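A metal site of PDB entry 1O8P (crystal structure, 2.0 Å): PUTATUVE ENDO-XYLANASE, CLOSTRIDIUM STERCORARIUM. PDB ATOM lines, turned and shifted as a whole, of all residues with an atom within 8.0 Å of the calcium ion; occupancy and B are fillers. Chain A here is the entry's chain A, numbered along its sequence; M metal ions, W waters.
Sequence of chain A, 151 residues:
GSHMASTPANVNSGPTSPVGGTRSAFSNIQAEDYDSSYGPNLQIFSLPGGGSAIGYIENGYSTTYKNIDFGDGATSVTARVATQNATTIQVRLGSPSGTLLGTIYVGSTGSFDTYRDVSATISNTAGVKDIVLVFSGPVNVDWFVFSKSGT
The backbone carbonyl oxygen (O) of Asp 142 sits close to the backbone NH (N) of Ala 31.
NH1 of Arg 80 is in salt-bridge range of OD2 of Asp 142.
Four residues have an atom within 4 Å of the calcium ion: Gln 30, Glu 32, Ser 52 and Asp 142.
The nearest printed residue that does not touch the calcium ion is Ala 31 (4.4 Å).
The calcium ion is bound by O of Ser 52 (2.4 Å), OD1 of Asp 142 (2.4 Å), OE1 of Gln 30 (2.4 Å), water W1 (2.4 Å), O of Asp 142 (2.5 Å), OE1 of Glu 32 (2.6 Å) and OE2 of Glu 32 (2.9 Å).
The calcium ion has seven donor atoms within binding distance.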
ATOM      1  N   ASN A  28       4.388  18.497  20.884  1.00  0.00           N
ATOM      2  CA  ASN A  28       5.641  17.745  20.921  1.00  0.00           C
ATOM      3  C   ASN A  28       6.828  18.519  20.401  1.00  0.00           C
ATOM      4  O   ASN A  28       6.823  19.072  19.287  1.00  0.00           O
ATOM      5  CB  ASN A  28       5.531  16.436  20.143  1.00  0.00           C
ATOM      6  CG  ASN A  28       4.478  15.525  20.721  1.00  0.00           C
ATOM      7  OD1 ASN A  28       3.940  15.799  21.781  1.00  0.00           O
ATOM      8  ND2 ASN A  28       4.153  14.492  20.014  1.00  0.00           N
ATOM      9  N   ILE A  29       7.847  18.603  21.240  1.00  0.00           N
ATOM     10  CA  ILE A  29       9.131  19.111  20.782  1.00  0.00           C
ATOM     11  C   ILE A  29       9.972  17.933  20.358  1.00  0.00           C
ATOM     12  O   ILE A  29      10.292  17.067  21.191  1.00  0.00           O
ATOM     13  CB  ILE A  29       9.846  19.956  21.888  1.00  0.00           C
ATOM     14  CG1 ILE A  29       8.922  21.058  22.407  1.00  0.00           C
ATOM     15  CG2 ILE A  29      11.155  20.552  21.319  1.00  0.00           C
ATOM     16  CD1 ILE A  29       9.169  21.455  23.840  1.00  0.00           C
ATOM     17  N   GLN A  30      10.332  17.903  19.070  1.00  0.00           N
ATOM     18  CA  GLN A  30      11.081  16.771  18.546  1.00  0.00           C
ATOM     19  C   GLN A  30      12.462  16.911  19.125  1.00  0.00           C
ATOM     20  O   GLN A  30      13.077  17.960  19.003  1.00  0.00           O
ATOM     21  CB  GLN A  30      11.057  16.731  16.997  1.00  0.00           C
ATOM     22  CG  GLN A  30       9.645  16.536  16.385  1.00  0.00           C
ATOM     23  CD  GLN A  30       8.962  15.245  16.887  1.00  0.00           C
ATOM     24  OE1 GLN A  30       9.648  14.246  17.186  1.00  0.00           O
ATOM     25  NE2 GLN A  30       7.639  15.276  17.003  1.00  0.00           N
ATOM     26  N   ALA A  31      12.954  15.858  19.789  1.00  0.00           N
ATOM     27  CA  ALA A  31      14.194  15.971  20.527  1.00  0.00           C
ATOM     28  C   ALA A  31      15.394  16.180  19.578  1.00  0.00           C
ATOM     29  O   ALA A  31      16.435  16.759  19.977  1.00  0.00           O
ATOM     30  CB  ALA A  31      14.388  14.729  21.405  1.00  0.00           C
ATOM     31  N   GLU A  32      15.264  15.698  18.349  1.00  0.00           N
ATOM     32  CA  GLU A  32      16.271  15.975  17.324  1.00  0.00           C
ATOM     33  C   GLU A  32      16.294  17.461  16.882  1.00  0.00           C
ATOM     34  O   GLU A  32      17.207  17.881  16.186  1.00  0.00           O
ATOM     35  CB  GLU A  32      16.129  15.027  16.097  1.00  0.00           C
ATOM     36  CG  GLU A  32      14.896  15.244  15.217  1.00  0.00           C
ATOM     37  CD  GLU A  32      13.667  14.535  15.753  1.00  0.00           C
ATOM     38  OE1 GLU A  32      13.591  14.259  16.974  1.00  0.00           O
ATOM     39  OE2 GLU A  32      12.746  14.272  14.970  1.00  0.00           O
ATOM     40  N   ASP A  33      15.304  18.261  17.291  1.00  0.00           N
ATOM     41  CA  ASP A  33      15.305  19.683  16.892  1.00  0.00           C
ATOM     42  C   ASP A  33      15.972  20.580  17.947  1.00  0.00           C
ATOM     43  O   ASP A  33      15.387  21.572  18.377  1.00  0.00           O
ATOM     44  CB  ASP A  33      13.889  20.177  16.631  1.00  0.00           C
ATOM     45  CG  ASP A  33      13.227  19.503  15.429  1.00  0.00           C
ATOM     46  OD1 ASP A  33      13.885  18.930  14.551  1.00  0.00           O
ATOM     47  OD2 ASP A  33      11.992  19.549  15.286  1.00  0.00           O
ATOM     48  N   ILE A  44      21.387  11.471  15.559  1.00  0.00           N
ATOM     49  CA  ILE A  44      19.964  11.304  15.290  1.00  0.00           C
ATOM     50  C   ILE A  44      19.784  10.030  14.497  1.00  0.00           C
ATOM     51  O   ILE A  44      20.472   9.815  13.494  1.00  0.00           O
ATOM     52  CB  ILE A  44      19.416  12.558  14.548  1.00  0.00           C
ATOM     53  CG1 ILE A  44      19.701  13.835  15.365  1.00  0.00           C
ATOM     54  CG2 ILE A  44      17.949  12.375  14.176  1.00  0.00           C
ATOM     55  CD1 ILE A  44      19.688  15.149  14.577  1.00  0.00           C
ATOM     56  N   PHE A  45      18.864   9.176  14.946  1.00  0.00           N
ATOM     57  CA  PHE A  45      18.587   7.901  14.327  1.00  0.00           C
ATOM     58  C   PHE A  45      17.175   7.887  13.765  1.00  0.00           C
ATOM     59  O   PHE A  45      16.247   8.406  14.402  1.00  0.00           O
ATOM     60  CB  PHE A  45      18.725   6.743  15.325  1.00  0.00           C
ATOM     61  CG  PHE A  45      20.085   6.617  15.933  1.00  0.00           C
ATOM     62  CD1 PHE A  45      21.213   6.497  15.114  1.00  0.00           C
ATOM     63  CD2 PHE A  45      20.233   6.575  17.316  1.00  0.00           C
ATOM     64  CE1 PHE A  45      22.473   6.407  15.650  1.00  0.00           C
ATOM     65  CE2 PHE A  45      21.510   6.465  17.864  1.00  0.00           C
ATOM     66  CZ  PHE A  45      22.624   6.405  17.010  1.00  0.00           C
ATOM     67  N   LEU A  47      13.632   6.108  12.926  1.00  0.00           N
ATOM     68  CA  LEU A  47      12.840   5.090  13.602  1.00  0.00           C
ATOM     69  C   LEU A  47      12.165   4.255  12.525  1.00  0.00           C
ATOM     70  O   LEU A  47      11.771   4.828  11.506  1.00  0.00           O
ATOM     71  CB  LEU A  47      11.796   5.733  14.535  1.00  0.00           C
ATOM     72  CG  LEU A  47      12.305   6.684  15.635  1.00  0.00           C
ATOM     73  CD1 LEU A  47      11.105   7.265  16.356  1.00  0.00           C
ATOM     74  CD2 LEU A  47      13.248   6.010  16.604  1.00  0.00           C
ATOM     75  N   GLY A  50       8.886   5.587  10.686  1.00  0.00           N
ATOM     76  CA  GLY A  50       8.909   7.038  10.444  1.00  0.00           C
ATOM     77  C   GLY A  50       9.326   7.856  11.674  1.00  0.00           C
ATOM     78  O   GLY A  50       9.035   7.497  12.823  1.00  0.00           O
ATOM     79  N   GLY A  51      10.005   8.971  11.451  1.00  0.00           N
ATOM     80  CA  GLY A  51      10.431   9.810  12.566  1.00  0.00           C
ATOM     81  C   GLY A  51      11.893   9.604  12.940  1.00  0.00           C
ATOM     82  O   GLY A  51      12.647   8.865  12.265  1.00  0.00           O
ATOM     83  N   SER A  52      12.322  10.307  13.973  1.00  0.00           N
ATOM     84  CA  SER A  52      13.715  10.254  14.415  1.00  0.00           C
ATOM     85  C   SER A  52      13.830  10.417  15.920  1.00  0.00           C
ATOM     86  O   SER A  52      12.919  10.926  16.552  1.00  0.00           O
ATOM     87  CB  SER A  52      14.562  11.359  13.755  1.00  0.00           C
ATOM     88  OG  SER A  52      14.520  11.304  12.350  1.00  0.00           O
ATOM     89  N   ALA A  53      14.963  10.003  16.485  1.00  0.00           N
ATOM     90  CA  ALA A  53      15.183  10.152  17.900  1.00  0.00           C
ATOM     91  C   ALA A  53      16.644  10.471  18.097  1.00  0.00           C
ATOM     92  O   ALA A  53      17.488  10.117  17.291  1.00  0.00           O
ATOM     93  CB  ALA A  53      14.780   8.888  18.650  1.00  0.00           C
ATOM     94  N   ILE A  54      16.965  11.215  19.132  1.00  0.00           N
ATOM     95  CA  ILE A  54      18.365  11.327  19.497  1.00  0.00           C
ATOM     96  C   ILE A  54      18.797  10.057  20.277  1.00  0.00           C
ATOM     97  O   ILE A  54      17.990   9.444  20.973  1.00  0.00           O
ATOM     98  CB  ILE A  54      18.628  12.652  20.239  1.00  0.00           C
ATOM     99  CG1 ILE A  54      17.758  12.751  21.533  1.00  0.00           C
ATOM    100  CG2 ILE A  54      18.360  13.848  19.252  1.00  0.00           C
ATOM    101  CD1 ILE A  54      17.974  13.984  22.395  1.00  0.00           C
ATOM    102  N   ARG A  80       9.015  10.746  25.206  1.00  0.00           N
ATOM    103  CA  ARG A  80       8.869   9.427  24.585  1.00  0.00           C
ATOM    104  C   ARG A  80      10.276   8.921  24.454  1.00  0.00           C
ATOM    105  O   ARG A  80      11.086   9.538  23.725  1.00  0.00           O
ATOM    106  CB  ARG A  80       8.218   9.497  23.197  1.00  0.00           C
ATOM    107  CG  ARG A  80       7.859   8.125  22.637  1.00  0.00           C
ATOM    108  CD  ARG A  80       7.031   8.120  21.345  1.00  0.00           C
ATOM    109  NE  ARG A  80       6.768   6.770  20.787  1.00  0.00           N
ATOM    110  CZ  ARG A  80       7.423   6.198  19.723  1.00  0.00           C
ATOM    111  NH1 ARG A  80       8.447   6.802  19.114  1.00  0.00           N
ATOM    112  NH2 ARG A  80       7.075   4.975  19.299  1.00  0.00           N
ATOM    113  N   TYR A 115       9.824   2.336  22.713  1.00  0.00           N
ATOM    114  CA  TYR A 115       9.548   3.657  23.291  1.00  0.00           C
ATOM    115  C   TYR A 115       8.335   3.636  24.200  1.00  0.00           C
ATOM    116  O   TYR A 115       7.332   2.974  23.914  1.00  0.00           O
ATOM    117  CB  TYR A 115       9.397   4.736  22.210  1.00  0.00           C
ATOM    118  CG  TYR A 115      10.727   5.032  21.533  1.00  0.00           C
ATOM    119  CD1 TYR A 115      11.225   4.205  20.539  1.00  0.00           C
ATOM    120  CD2 TYR A 115      11.520   6.116  21.944  1.00  0.00           C
ATOM    121  CE1 TYR A 115      12.455   4.440  19.954  1.00  0.00           C
ATOM    122  CE2 TYR A 115      12.764   6.364  21.343  1.00  0.00           C
ATOM    123  CZ  TYR A 115      13.217   5.536  20.360  1.00  0.00           C
ATOM    124  OH  TYR A 115      14.428   5.782  19.735  1.00  0.00           O
ATOM    125  N   VAL A 141      15.581   9.570  22.812  1.00  0.00           N
ATOM    126  CA  VAL A 141      14.491  10.488  23.012  1.00  0.00           C
ATOM    127  C   VAL A 141      13.915  10.854  21.661  1.00  0.00           C
ATOM    128  O   VAL A 141      14.606  11.399  20.808  1.00  0.00           O
ATOM    129  CB  VAL A 141      14.907  11.757  23.766  1.00  0.00           C
ATOM    130  CG1 VAL A 141      13.632  12.534  24.256  1.00  0.00           C
ATOM    131  CG2 VAL A 141      15.866  11.434  24.968  1.00  0.00           C
ATOM    132  N   ASP A 142      12.637  10.514  21.474  1.00  0.00           N
ATOM    133  CA  ASP A 142      11.903  10.806  20.242  1.00  0.00           C
ATOM    134  C   ASP A 142      11.441  12.267  20.356  1.00  0.00           C
ATOM    135  O   ASP A 142      11.803  13.096  19.545  1.00  0.00           O
ATOM    136  CB  ASP A 142      10.738   9.836  20.099  1.00  0.00           C
ATOM    137  CG  ASP A 142       9.959  10.020  18.849  1.00  0.00           C
ATOM    138  OD1 ASP A 142      10.241  10.946  18.026  1.00  0.00           O
ATOM    139  OD2 ASP A 142       9.005   9.270  18.603  1.00  0.00           O
ATOM    140  N   TRP A 143      10.667  12.577  21.404  1.00  0.00           N
ATOM    141  CA  TRP A 143      10.158  13.916  21.620  1.00  0.00           C
ATOM    142  C   TRP A 143       9.840  14.109  23.074  1.00  0.00           C
ATOM    143  O   TRP A 143       9.861  13.129  23.853  1.00  0.00           O
ATOM    144  CB  TRP A 143       8.900  14.224  20.760  1.00  0.00           C
ATOM    145  CG  TRP A 143       7.808  13.199  20.781  1.00  0.00           C
ATOM    146  CD1 TRP A 143       7.479  12.336  19.745  1.00  0.00           C
ATOM    147  CD2 TRP A 143       6.858  12.946  21.832  1.00  0.00           C
ATOM    148  NE1 TRP A 143       6.395  11.565  20.104  1.00  0.00           N
ATOM    149  CE2 TRP A 143       5.990  11.904  21.377  1.00  0.00           C
ATOM    150  CE3 TRP A 143       6.628  13.484  23.107  1.00  0.00           C
ATOM    151  CZ2 TRP A 143       4.933  11.381  22.175  1.00  0.00           C
ATOM    152  CZ3 TRP A 143       5.598  12.966  23.908  1.00  0.00           C
ATOM    153  CH2 TRP A 143       4.752  11.932  23.434  1.00  0.00           C
ATOM    154  N   PHE A 144       9.556  15.361  23.425  1.00  0.00           N
ATOM    155  CA  PHE A 144       9.091  15.724  24.759  1.00  0.00           C
ATOM    156  C   PHE A 144       8.066  16.850  24.664  1.00  0.00           C
ATOM    157  O   PHE A 144       7.997  17.579  23.667  1.00  0.00           O
ATOM    158  CB  PHE A 144      10.256  16.040  25.747  1.00  0.00           C
ATOM    159  CG  PHE A 144      11.014  17.305  25.474  1.00  0.00           C
ATOM    160  CD1 PHE A 144      11.953  17.374  24.418  1.00  0.00           C
ATOM    161  CD2 PHE A 144      10.859  18.421  26.289  1.00  0.00           C
ATOM    162  CE1 PHE A 144      12.684  18.547  24.148  1.00  0.00           C
ATOM    163  CE2 PHE A 144      11.604  19.601  26.012  1.00  0.00           C
ATOM    164  CZ  PHE A 144      12.509  19.653  24.958  1.00  0.00           C
HETATM  165 CA    CA M   1      11.511  12.736  17.074  1.00  0.00          CA
HETATM  166  O   HOH W   1      10.682  12.531  14.778  1.00  0.00           O
